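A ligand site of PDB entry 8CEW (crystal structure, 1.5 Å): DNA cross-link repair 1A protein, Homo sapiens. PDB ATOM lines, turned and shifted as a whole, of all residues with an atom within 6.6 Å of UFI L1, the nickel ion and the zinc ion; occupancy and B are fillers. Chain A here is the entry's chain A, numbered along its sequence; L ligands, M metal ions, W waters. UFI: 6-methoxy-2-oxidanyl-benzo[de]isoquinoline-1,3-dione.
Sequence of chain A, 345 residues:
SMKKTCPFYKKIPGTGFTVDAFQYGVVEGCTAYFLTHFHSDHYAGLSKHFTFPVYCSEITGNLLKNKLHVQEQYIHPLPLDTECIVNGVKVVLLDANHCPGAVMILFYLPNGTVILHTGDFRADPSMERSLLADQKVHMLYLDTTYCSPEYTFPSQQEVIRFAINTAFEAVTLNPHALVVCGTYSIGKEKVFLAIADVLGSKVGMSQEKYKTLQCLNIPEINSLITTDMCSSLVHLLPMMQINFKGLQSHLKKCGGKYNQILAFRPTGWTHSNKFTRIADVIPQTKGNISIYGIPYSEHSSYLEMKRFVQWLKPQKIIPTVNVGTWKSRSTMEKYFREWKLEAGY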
ATOM      1  N   HIS A  37     -16.016  -2.222  -8.870  1.00  0.00           N
ATOM      2  CA  HIS A  37     -17.395  -1.730  -8.820  1.00  0.00           C
ATOM      3  C   HIS A  37     -17.427  -0.229  -9.092  1.00  0.00           C
ATOM      4  O   HIS A  37     -16.401   0.458  -9.001  1.00  0.00           O
ATOM      5  CB  HIS A  37     -18.073  -2.042  -7.479  1.00  0.00           C
ATOM      6  CG  HIS A  37     -17.486  -1.362  -6.277  1.00  0.00           C
ATOM      7  ND1 HIS A  37     -16.189  -1.572  -5.834  1.00  0.00           N
ATOM      8  CD2 HIS A  37     -18.052  -0.528  -5.370  1.00  0.00           C
ATOM      9  CE1 HIS A  37     -15.977  -0.877  -4.735  1.00  0.00           C
ATOM     10  NE2 HIS A  37     -17.094  -0.234  -4.426  1.00  0.00           N
ATOM     11  N   PHE A  38     -18.622   0.265  -9.414  1.00  0.00           N
ATOM     12  CA  PHE A  38     -18.810   1.657  -9.836  1.00  0.00           C
ATOM     13  C   PHE A  38     -19.112   2.552  -8.626  1.00  0.00           C
ATOM     14  O   PHE A  38     -20.224   3.047  -8.429  1.00  0.00           O
ATOM     15  CB  PHE A  38     -19.910   1.746 -10.886  1.00  0.00           C
ATOM     16  CG  PHE A  38     -19.957   3.059 -11.612  1.00  0.00           C
ATOM     17  CD1 PHE A  38     -19.056   3.348 -12.628  1.00  0.00           C
ATOM     18  CD2 PHE A  38     -20.897   4.016 -11.284  1.00  0.00           C
ATOM     19  CE1 PHE A  38     -19.099   4.560 -13.304  1.00  0.00           C
ATOM     20  CE2 PHE A  38     -20.955   5.234 -11.948  1.00  0.00           C
ATOM     21  CZ  PHE A  38     -20.048   5.506 -12.949  1.00  0.00           C
ATOM     22  N   HIS A  39     -18.081   2.743  -7.803  1.00  0.00           N
ATOM     23  CA  HIS A  39     -18.112   3.700  -6.698  1.00  0.00           C
ATOM     24  C   HIS A  39     -16.955   4.685  -6.859  1.00  0.00           C
ATOM     25  O   HIS A  39     -15.870   4.325  -7.312  1.00  0.00           O
ATOM     26  CB  HIS A  39     -18.002   3.015  -5.326  1.00  0.00           C
ATOM     27  CG  HIS A  39     -19.313   2.574  -4.774  1.00  0.00           C
ATOM     28  ND1 HIS A  39     -19.413   1.707  -3.715  1.00  0.00           N
ATOM     29  CD2 HIS A  39     -20.585   2.884  -5.127  1.00  0.00           C
ATOM     30  CE1 HIS A  39     -20.693   1.498  -3.433  1.00  0.00           C
ATOM     31  NE2 HIS A  39     -21.426   2.205  -4.272  1.00  0.00           N
ATOM     32  N   SER A  40     -17.201   5.920  -6.414  1.00  0.00           N
ATOM     33  CA  SER A  40     -16.349   7.054  -6.815  1.00  0.00           C
ATOM     34  C   SER A  40     -14.915   6.889  -6.337  1.00  0.00           C
ATOM     35  O   SER A  40     -13.973   7.215  -7.065  1.00  0.00           O
ATOM     36  CB  SER A  40     -16.948   8.354  -6.273  1.00  0.00           C
ATOM     37  OG  SER A  40     -17.116   8.291  -4.862  1.00  0.00           O
ATOM     38  N   ASP A  41     -14.710   6.381  -5.110  1.00  0.00           N
ATOM     39  CA  ASP A  41     -13.353   6.211  -4.620  1.00  0.00           C
ATOM     40  C   ASP A  41     -12.602   5.096  -5.342  1.00  0.00           C
ATOM     41  O   ASP A  41     -11.384   4.956  -5.153  1.00  0.00           O
ATOM     42  CB  ASP A  41     -13.366   5.931  -3.115  1.00  0.00           C
ATOM     43  CG  ASP A  41     -12.343   6.760  -2.355  1.00  0.00           C
ATOM     44  OD1 ASP A  41     -12.316   7.987  -2.564  1.00  0.00           O
ATOM     45  OD2 ASP A  41     -11.597   6.188  -1.545  1.00  0.00           O
ATOM     46  N   HIS A  42     -13.287   4.335  -6.184  1.00  0.00           N
ATOM     47  CA  HIS A  42     -12.685   3.205  -6.876  1.00  0.00           C
ATOM     48  C   HIS A  42     -12.505   3.436  -8.364  1.00  0.00           C
ATOM     49  O   HIS A  42     -11.483   3.023  -8.923  1.00  0.00           O
ATOM     50  CB  HIS A  42     -13.533   1.943  -6.628  1.00  0.00           C
ATOM     51  CG  HIS A  42     -13.613   1.581  -5.174  1.00  0.00           C
ATOM     52  ND1 HIS A  42     -12.818   0.616  -4.613  1.00  0.00           N
ATOM     53  CD2 HIS A  42     -14.370   2.092  -4.174  1.00  0.00           C
ATOM     54  CE1 HIS A  42     -13.091   0.525  -3.317  1.00  0.00           C
ATOM     55  NE2 HIS A  42     -14.026   1.415  -3.030  1.00  0.00           N
ATOM     56  N   HIS A  98     -22.069  -6.268  -2.427  1.00  0.00           N
ATOM     57  CA  HIS A  98     -21.823  -4.872  -2.109  1.00  0.00           C
ATOM     58  C   HIS A  98     -22.923  -4.088  -2.794  1.00  0.00           C
ATOM     59  O   HIS A  98     -24.091  -4.151  -2.365  1.00  0.00           O
ATOM     60  CB  HIS A  98     -20.391  -4.498  -2.515  1.00  0.00           C
ATOM     61  CG  HIS A  98     -19.967  -3.101  -2.175  1.00  0.00           C
ATOM     62  ND1 HIS A  98     -20.059  -2.574  -0.898  1.00  0.00           N
ATOM     63  CD2 HIS A  98     -19.407  -2.130  -2.940  1.00  0.00           C
ATOM     64  CE1 HIS A  98     -19.592  -1.333  -0.902  1.00  0.00           C
ATOM     65  NE2 HIS A  98     -19.179  -1.042  -2.120  1.00  0.00           N
ATOM     66  N   CYS A  99     -22.635  -3.412  -3.889  1.00  0.00           N
ATOM     67  CA  CYS A  99     -23.612  -2.700  -4.701  1.00  0.00           C
ATOM     68  C   CYS A  99     -23.802  -3.445  -6.017  1.00  0.00           C
ATOM     69  O   CYS A  99     -23.070  -4.393  -6.327  1.00  0.00           O
ATOM     70  CB  CYS A  99     -23.137  -1.264  -4.952  1.00  0.00           C
ATOM     71  SG  CYS A  99     -21.626  -1.172  -5.916  1.00  0.00           S
ATOM     72  N   ASP A 120     -14.733  -4.111  -2.577  1.00  0.00           N
ATOM     73  CA  ASP A 120     -15.611  -3.854  -1.441  1.00  0.00           C
ATOM     74  C   ASP A 120     -16.619  -5.003  -1.355  1.00  0.00           C
ATOM     75  O   ASP A 120     -17.208  -5.375  -2.373  1.00  0.00           O
ATOM     76  CB  ASP A 120     -16.359  -2.537  -1.603  1.00  0.00           C
ATOM     77  CG  ASP A 120     -15.528  -1.323  -1.235  1.00  0.00           C
ATOM     78  OD1 ASP A 120     -14.388  -1.488  -0.750  1.00  0.00           O
ATOM     79  OD2 ASP A 120     -16.035  -0.204  -1.433  1.00  0.00           O
ATOM     80  N   ASP A 143     -11.106  -6.189   2.024  1.00  0.00           N
ATOM     81  CA  ASP A 143     -11.881  -5.001   2.427  1.00  0.00           C
ATOM     82  C   ASP A 143     -12.018  -4.995   3.948  1.00  0.00           C
ATOM     83  O   ASP A 143     -12.866  -5.695   4.514  1.00  0.00           O
ATOM     84  CB  ASP A 143     -13.240  -5.019   1.743  1.00  0.00           C
ATOM     85  CG  ASP A 143     -14.201  -3.968   2.284  1.00  0.00           C
ATOM     86  OD1 ASP A 143     -13.754  -3.029   2.975  1.00  0.00           O
ATOM     87  OD2 ASP A 143     -15.413  -4.073   2.011  1.00  0.00           O
ATOM     88  N   THR A 145     -12.789  -2.318   5.856  1.00  0.00           N
ATOM     89  CA  THR A 145     -13.485  -1.092   6.251  1.00  0.00           C
ATOM     90  C   THR A 145     -13.868  -1.094   7.740  1.00  0.00           C
ATOM     91  O   THR A 145     -13.568  -0.136   8.465  1.00  0.00           O
ATOM     92  CB  THR A 145     -14.724  -0.895   5.385  1.00  0.00           C
ATOM     93  OG1 THR A 145     -14.330  -0.699   4.020  1.00  0.00           O
ATOM     94  CG2 THR A 145     -15.526   0.311   5.844  1.00  0.00           C
ATOM     95  N   TYR A 184     -26.615   8.705  -2.950  1.00  0.00           N
ATOM     96  CA  TYR A 184     -25.579   9.298  -3.802  1.00  0.00           C
ATOM     97  C   TYR A 184     -24.973   8.233  -4.702  1.00  0.00           C
ATOM     98  O   TYR A 184     -25.160   8.257  -5.924  1.00  0.00           O
ATOM     99  CB  TYR A 184     -24.489  10.010  -2.979  1.00  0.00           C
ATOM    100  CG  TYR A 184     -24.109   9.441  -1.614  1.00  0.00           C
ATOM    101  CD1 TYR A 184     -23.735   8.112  -1.449  1.00  0.00           C
ATOM    102  CD2 TYR A 184     -24.034  10.270  -0.506  1.00  0.00           C
ATOM    103  CE1 TYR A 184     -23.374   7.621  -0.216  1.00  0.00           C
ATOM    104  CE2 TYR A 184     -23.669   9.787   0.729  1.00  0.00           C
ATOM    105  CZ  TYR A 184     -23.339   8.462   0.874  1.00  0.00           C
ATOM    106  OH  TYR A 184     -22.962   7.973   2.109  1.00  0.00           O
ATOM    107  N   SER A 185     -24.272   7.280  -4.109  1.00  0.00           N
ATOM    108  CA  SER A 185     -23.693   6.186  -4.872  1.00  0.00           C
ATOM    109  C   SER A 185     -24.773   5.159  -5.177  1.00  0.00           C
ATOM    110  O   SER A 185     -25.803   5.073  -4.496  1.00  0.00           O
ATOM    111  CB  SER A 185     -22.554   5.540  -4.098  1.00  0.00           C
ATOM    112  OG  SER A 185     -21.721   6.519  -3.485  1.00  0.00           O
ATOM    113  N   ILE A 186     -24.520   4.358  -6.220  1.00  0.00           N
ATOM    114  CA  ILE A 186     -25.320   3.155  -6.391  1.00  0.00           C
ATOM    115  C   ILE A 186     -25.156   2.288  -5.156  1.00  0.00           C
ATOM    116  O   ILE A 186     -24.242   2.474  -4.334  1.00  0.00           O
ATOM    117  CB  ILE A 186     -24.916   2.387  -7.670  1.00  0.00           C
ATOM    118  CG1 ILE A 186     -23.497   1.833  -7.541  1.00  0.00           C
ATOM    119  CG2 ILE A 186     -25.008   3.300  -8.864  1.00  0.00           C
ATOM    120  CD1 ILE A 186     -23.112   0.879  -8.667  1.00  0.00           C
ATOM    121  N   LYS A 188     -27.709  -0.004  -2.081  1.00  0.00           N
ATOM    122  CA  LYS A 188     -28.784   0.214  -1.109  1.00  0.00           C
ATOM    123  C   LYS A 188     -30.129   0.496  -1.774  1.00  0.00           C
ATOM    124  O   LYS A 188     -31.035   1.053  -1.139  1.00  0.00           O
ATOM    125  CB  LYS A 188     -28.400   1.327  -0.118  1.00  0.00           C
ATOM    126  CG  LYS A 188     -26.999   1.131   0.461  1.00  0.00           C
ATOM    127  CD  LYS A 188     -26.615   2.152   1.523  1.00  0.00           C
ATOM    128  CE  LYS A 188     -25.190   1.887   2.006  1.00  0.00           C
ATOM    129  NZ  LYS A 188     -24.850   2.692   3.209  1.00  0.00           N
ATOM    130  N   GLY A 268     -23.796   3.930   6.702  1.00  0.00           N
ATOM    131  CA  GLY A 268     -23.078   2.752   7.122  1.00  0.00           C
ATOM    132  C   GLY A 268     -23.209   2.609   8.624  1.00  0.00           C
ATOM    133  O   GLY A 268     -24.292   2.801   9.185  1.00  0.00           O
ATOM    134  N   GLU A 298     -23.362  -2.019   3.265  1.00  0.00           N
ATOM    135  CA  GLU A 298     -22.933  -2.928   2.213  1.00  0.00           C
ATOM    136  C   GLU A 298     -21.458  -3.335   2.383  1.00  0.00           C
ATOM    137  O   GLU A 298     -20.836  -3.789   1.428  1.00  0.00           O
ATOM    138  CB  GLU A 298     -23.212  -2.311   0.843  1.00  0.00           C
ATOM    139  CG  GLU A 298     -24.737  -2.265   0.565  1.00  0.00           C
ATOM    140  CD  GLU A 298     -25.131  -1.799  -0.832  1.00  0.00           C
ATOM    141  OE1 GLU A 298     -24.369  -1.060  -1.491  1.00  0.00           O
ATOM    142  OE2 GLU A 298     -26.246  -2.173  -1.280  1.00  0.00           O
ATOM    143  N   HIS A 299     -20.919  -3.184   3.599  1.00  0.00           N
ATOM    144  CA  HIS A 299     -19.612  -3.714   3.981  1.00  0.00           C
ATOM    145  C   HIS A 299     -19.787  -4.734   5.104  1.00  0.00           C
ATOM    146  O   HIS A 299     -20.745  -4.666   5.884  1.00  0.00           O
ATOM    147  CB  HIS A 299     -18.656  -2.609   4.455  1.00  0.00           C
ATOM    148  CG  HIS A 299     -18.164  -1.670   3.386  1.00  0.00           C
ATOM    149  ND1 HIS A 299     -17.082  -1.953   2.589  1.00  0.00           N
ATOM    150  CD2 HIS A 299     -18.565  -0.426   3.047  1.00  0.00           C
ATOM    151  CE1 HIS A 299     -16.865  -0.934   1.771  1.00  0.00           C
ATOM    152  NE2 HIS A 299     -17.753   0.005   2.025  1.00  0.00           N
ATOM    153  N   VAL A 321      -8.198  -1.196   3.036  1.00  0.00           N
ATOM    154  CA  VAL A 321      -8.890  -0.062   3.645  1.00  0.00           C
ATOM    155  C   VAL A 321      -8.284   0.187   5.028  1.00  0.00           C
ATOM    156  O   VAL A 321      -7.845  -0.759   5.704  1.00  0.00           O
ATOM    157  CB  VAL A 321     -10.419  -0.303   3.750  1.00  0.00           C
ATOM    158  CG1 VAL A 321     -11.139   0.920   4.335  1.00  0.00           C
ATOM    159  CG2 VAL A 321     -11.010  -0.667   2.389  1.00  0.00           C
HETATM  160  C1  UFI L   1     -19.662   9.899   0.612  1.00  0.00           C
HETATM  161  C10 UFI L   1     -20.937   4.529   1.351  1.00  0.00           C
HETATM  162  C11 UFI L   1     -20.683   5.853   1.128  1.00  0.00           C
HETATM  163  C12 UFI L   1     -19.704   6.260   0.189  1.00  0.00           C
HETATM  164  C13 UFI L   1     -19.003   5.262  -0.515  1.00  0.00           C
HETATM  165  C2  UFI L   1     -19.404   7.632  -0.067  1.00  0.00           C
HETATM  166  C3  UFI L   1     -18.431   7.959  -0.992  1.00  0.00           C
HETATM  167  C4  UFI L   1     -17.736   6.951  -1.683  1.00  0.00           C
HETATM  168  C5  UFI L   1     -18.021   5.632  -1.450  1.00  0.00           C
HETATM  169  C6  UFI L   1     -17.292   4.564  -2.171  1.00  0.00           C
HETATM  170  C7  UFI L   1     -18.523   2.879  -1.012  1.00  0.00           C
HETATM  171  C8  UFI L   1     -19.275   3.910  -0.268  1.00  0.00           C
HETATM  172  C9  UFI L   1     -20.236   3.544   0.640  1.00  0.00           C
HETATM  173  N1  UFI L   1     -17.530   3.265  -1.865  1.00  0.00           N
HETATM  174  O1  UFI L   1     -20.116   8.542   0.650  1.00  0.00           O
HETATM  175  O2  UFI L   1     -18.760   1.693  -0.847  1.00  0.00           O
HETATM  176  O3  UFI L   1     -16.754   2.287  -2.437  1.00  0.00           O
HETATM  177  O4  UFI L   1     -16.448   4.847  -3.015  1.00  0.00           O
HETATM  178  C1  UFI L   2     -15.203  10.573   0.991  1.00  0.00           C
HETATM  179  C10 UFI L   2     -18.190   6.756   3.771  1.00  0.00           C
HETATM  180  C11 UFI L   2     -17.480   7.700   3.086  1.00  0.00           C
HETATM  181  C12 UFI L   2     -16.589   7.338   2.058  1.00  0.00           C
HETATM  182  C13 UFI L   2     -16.451   5.972   1.740  1.00  0.00           C
HETATM  183  C2  UFI L   2     -15.821   8.292   1.325  1.00  0.00           C
HETATM  184  C3  UFI L   2     -14.973   7.870   0.322  1.00  0.00           C
HETATM  185  C4  UFI L   2     -14.844   6.506   0.024  1.00  0.00           C
HETATM  186  C5  UFI L   2     -15.568   5.567   0.722  1.00  0.00           C
HETATM  187  C6  UFI L   2     -15.446   4.129   0.402  1.00  0.00           C
HETATM  188  C7  UFI L   2     -17.032   3.586   2.098  1.00  0.00           C
HETATM  189  C8  UFI L   2     -17.191   5.006   2.447  1.00  0.00           C
HETATM  190  C9  UFI L   2     -18.053   5.402   3.446  1.00  0.00           C
HETATM  191  N1  UFI L   2     -16.201   3.234   1.078  1.00  0.00           N
HETATM  192  O1  UFI L   2     -15.998   9.608   1.670  1.00  0.00           O
HETATM  193  O2  UFI L   2     -17.664   2.725   2.706  1.00  0.00           O
HETATM  194  O3  UFI L   2     -16.125   1.909   0.705  1.00  0.00           O
HETATM  195  O4  UFI L   2     -14.706   3.749  -0.489  1.00  0.00           O
HETATM  196 NI    NI M   1     -17.929   0.654  -2.589  1.00  0.00          NI
HETATM  197 ZN    ZN M   2     -15.114   1.715  -1.173  1.00  0.00          ZN
HETATM  198  O   HOH W   1     -13.423   0.859  -0.128  1.00  0.00           O
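Of the 19 residues printed, 4 come within 4 Å of the nickel ion. The nearest printed residue that does not touch the nickel ion is His 42 (4.001 Å).
The nickel ion is bound by O3 of UFI L1 (2.0 Å). A ring nitrogen (ND1) of His 39 binds the nickel ion (2.1 Å). A ring nitrogen (NE2) of His 98 is bound to the nickel ion, at 2.2 Å. O2 of UFI L1 is bound to the nickel ion. The nickel ion is bound by a ring nitrogen (NE2) of His 37, 2.2 Å away. The side-chain carboxylate (OD2) of Asp 120 is bound to the nickel ion (2.4 Å).
N of Asp 41 is in hydrogen-bond range of O4 of UFI L1 (3.1 Å). O1 of UFI L1 lies close to OH of Tyr 184, 3.2 Å away. An oxygen (O2) of UFI L1 sits close to a ring nitrogen (NE2) of His 299 (3.5 Å). A ring nitrogen (NE2) of His 299 sits at hydrogen-bond distance from an oxygen (O2) of UFI L2 (2.8 Å).
OG of Ser 40 touches C4 of UFI L1, at 3.5 Å. Along chain A the residues within 4 Å of UFI L1 span positions 37 to 299.
The zinc ion is bound by O3 of UFI L2 (2.1 Å), OD2 of Asp 120 (2.1 Å), O3 of UFI L1 (2.1 Å), water W1 (2.2 Å), NE2 of His 42 (2.2 Å) and O4 of UFI L2 (2.2 Å).
The side-chain sulfur (SG) of Cys 99 sits at hydrogen-bond distance from a ring nitrogen (NE2) of His 39, 3.8 Å away. O of Ile 186 sits at hydrogen-bond distance from NE2 of His 39 (2.8 Å). A ring nitrogen (ND1) of His 98 sits at hydrogen-bond distance from the backbone carbonyl oxygen (O) of Glu 298. ND1 of His 299 sits at hydrogen-bond distance from OG1 of Thr 145, at 3.3 Å. A ring nitrogen (ND1) of His 299 lies within hydrogen-bond range of the side-chain carboxylate (OD2) of Asp 143, at 2.8 Å.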
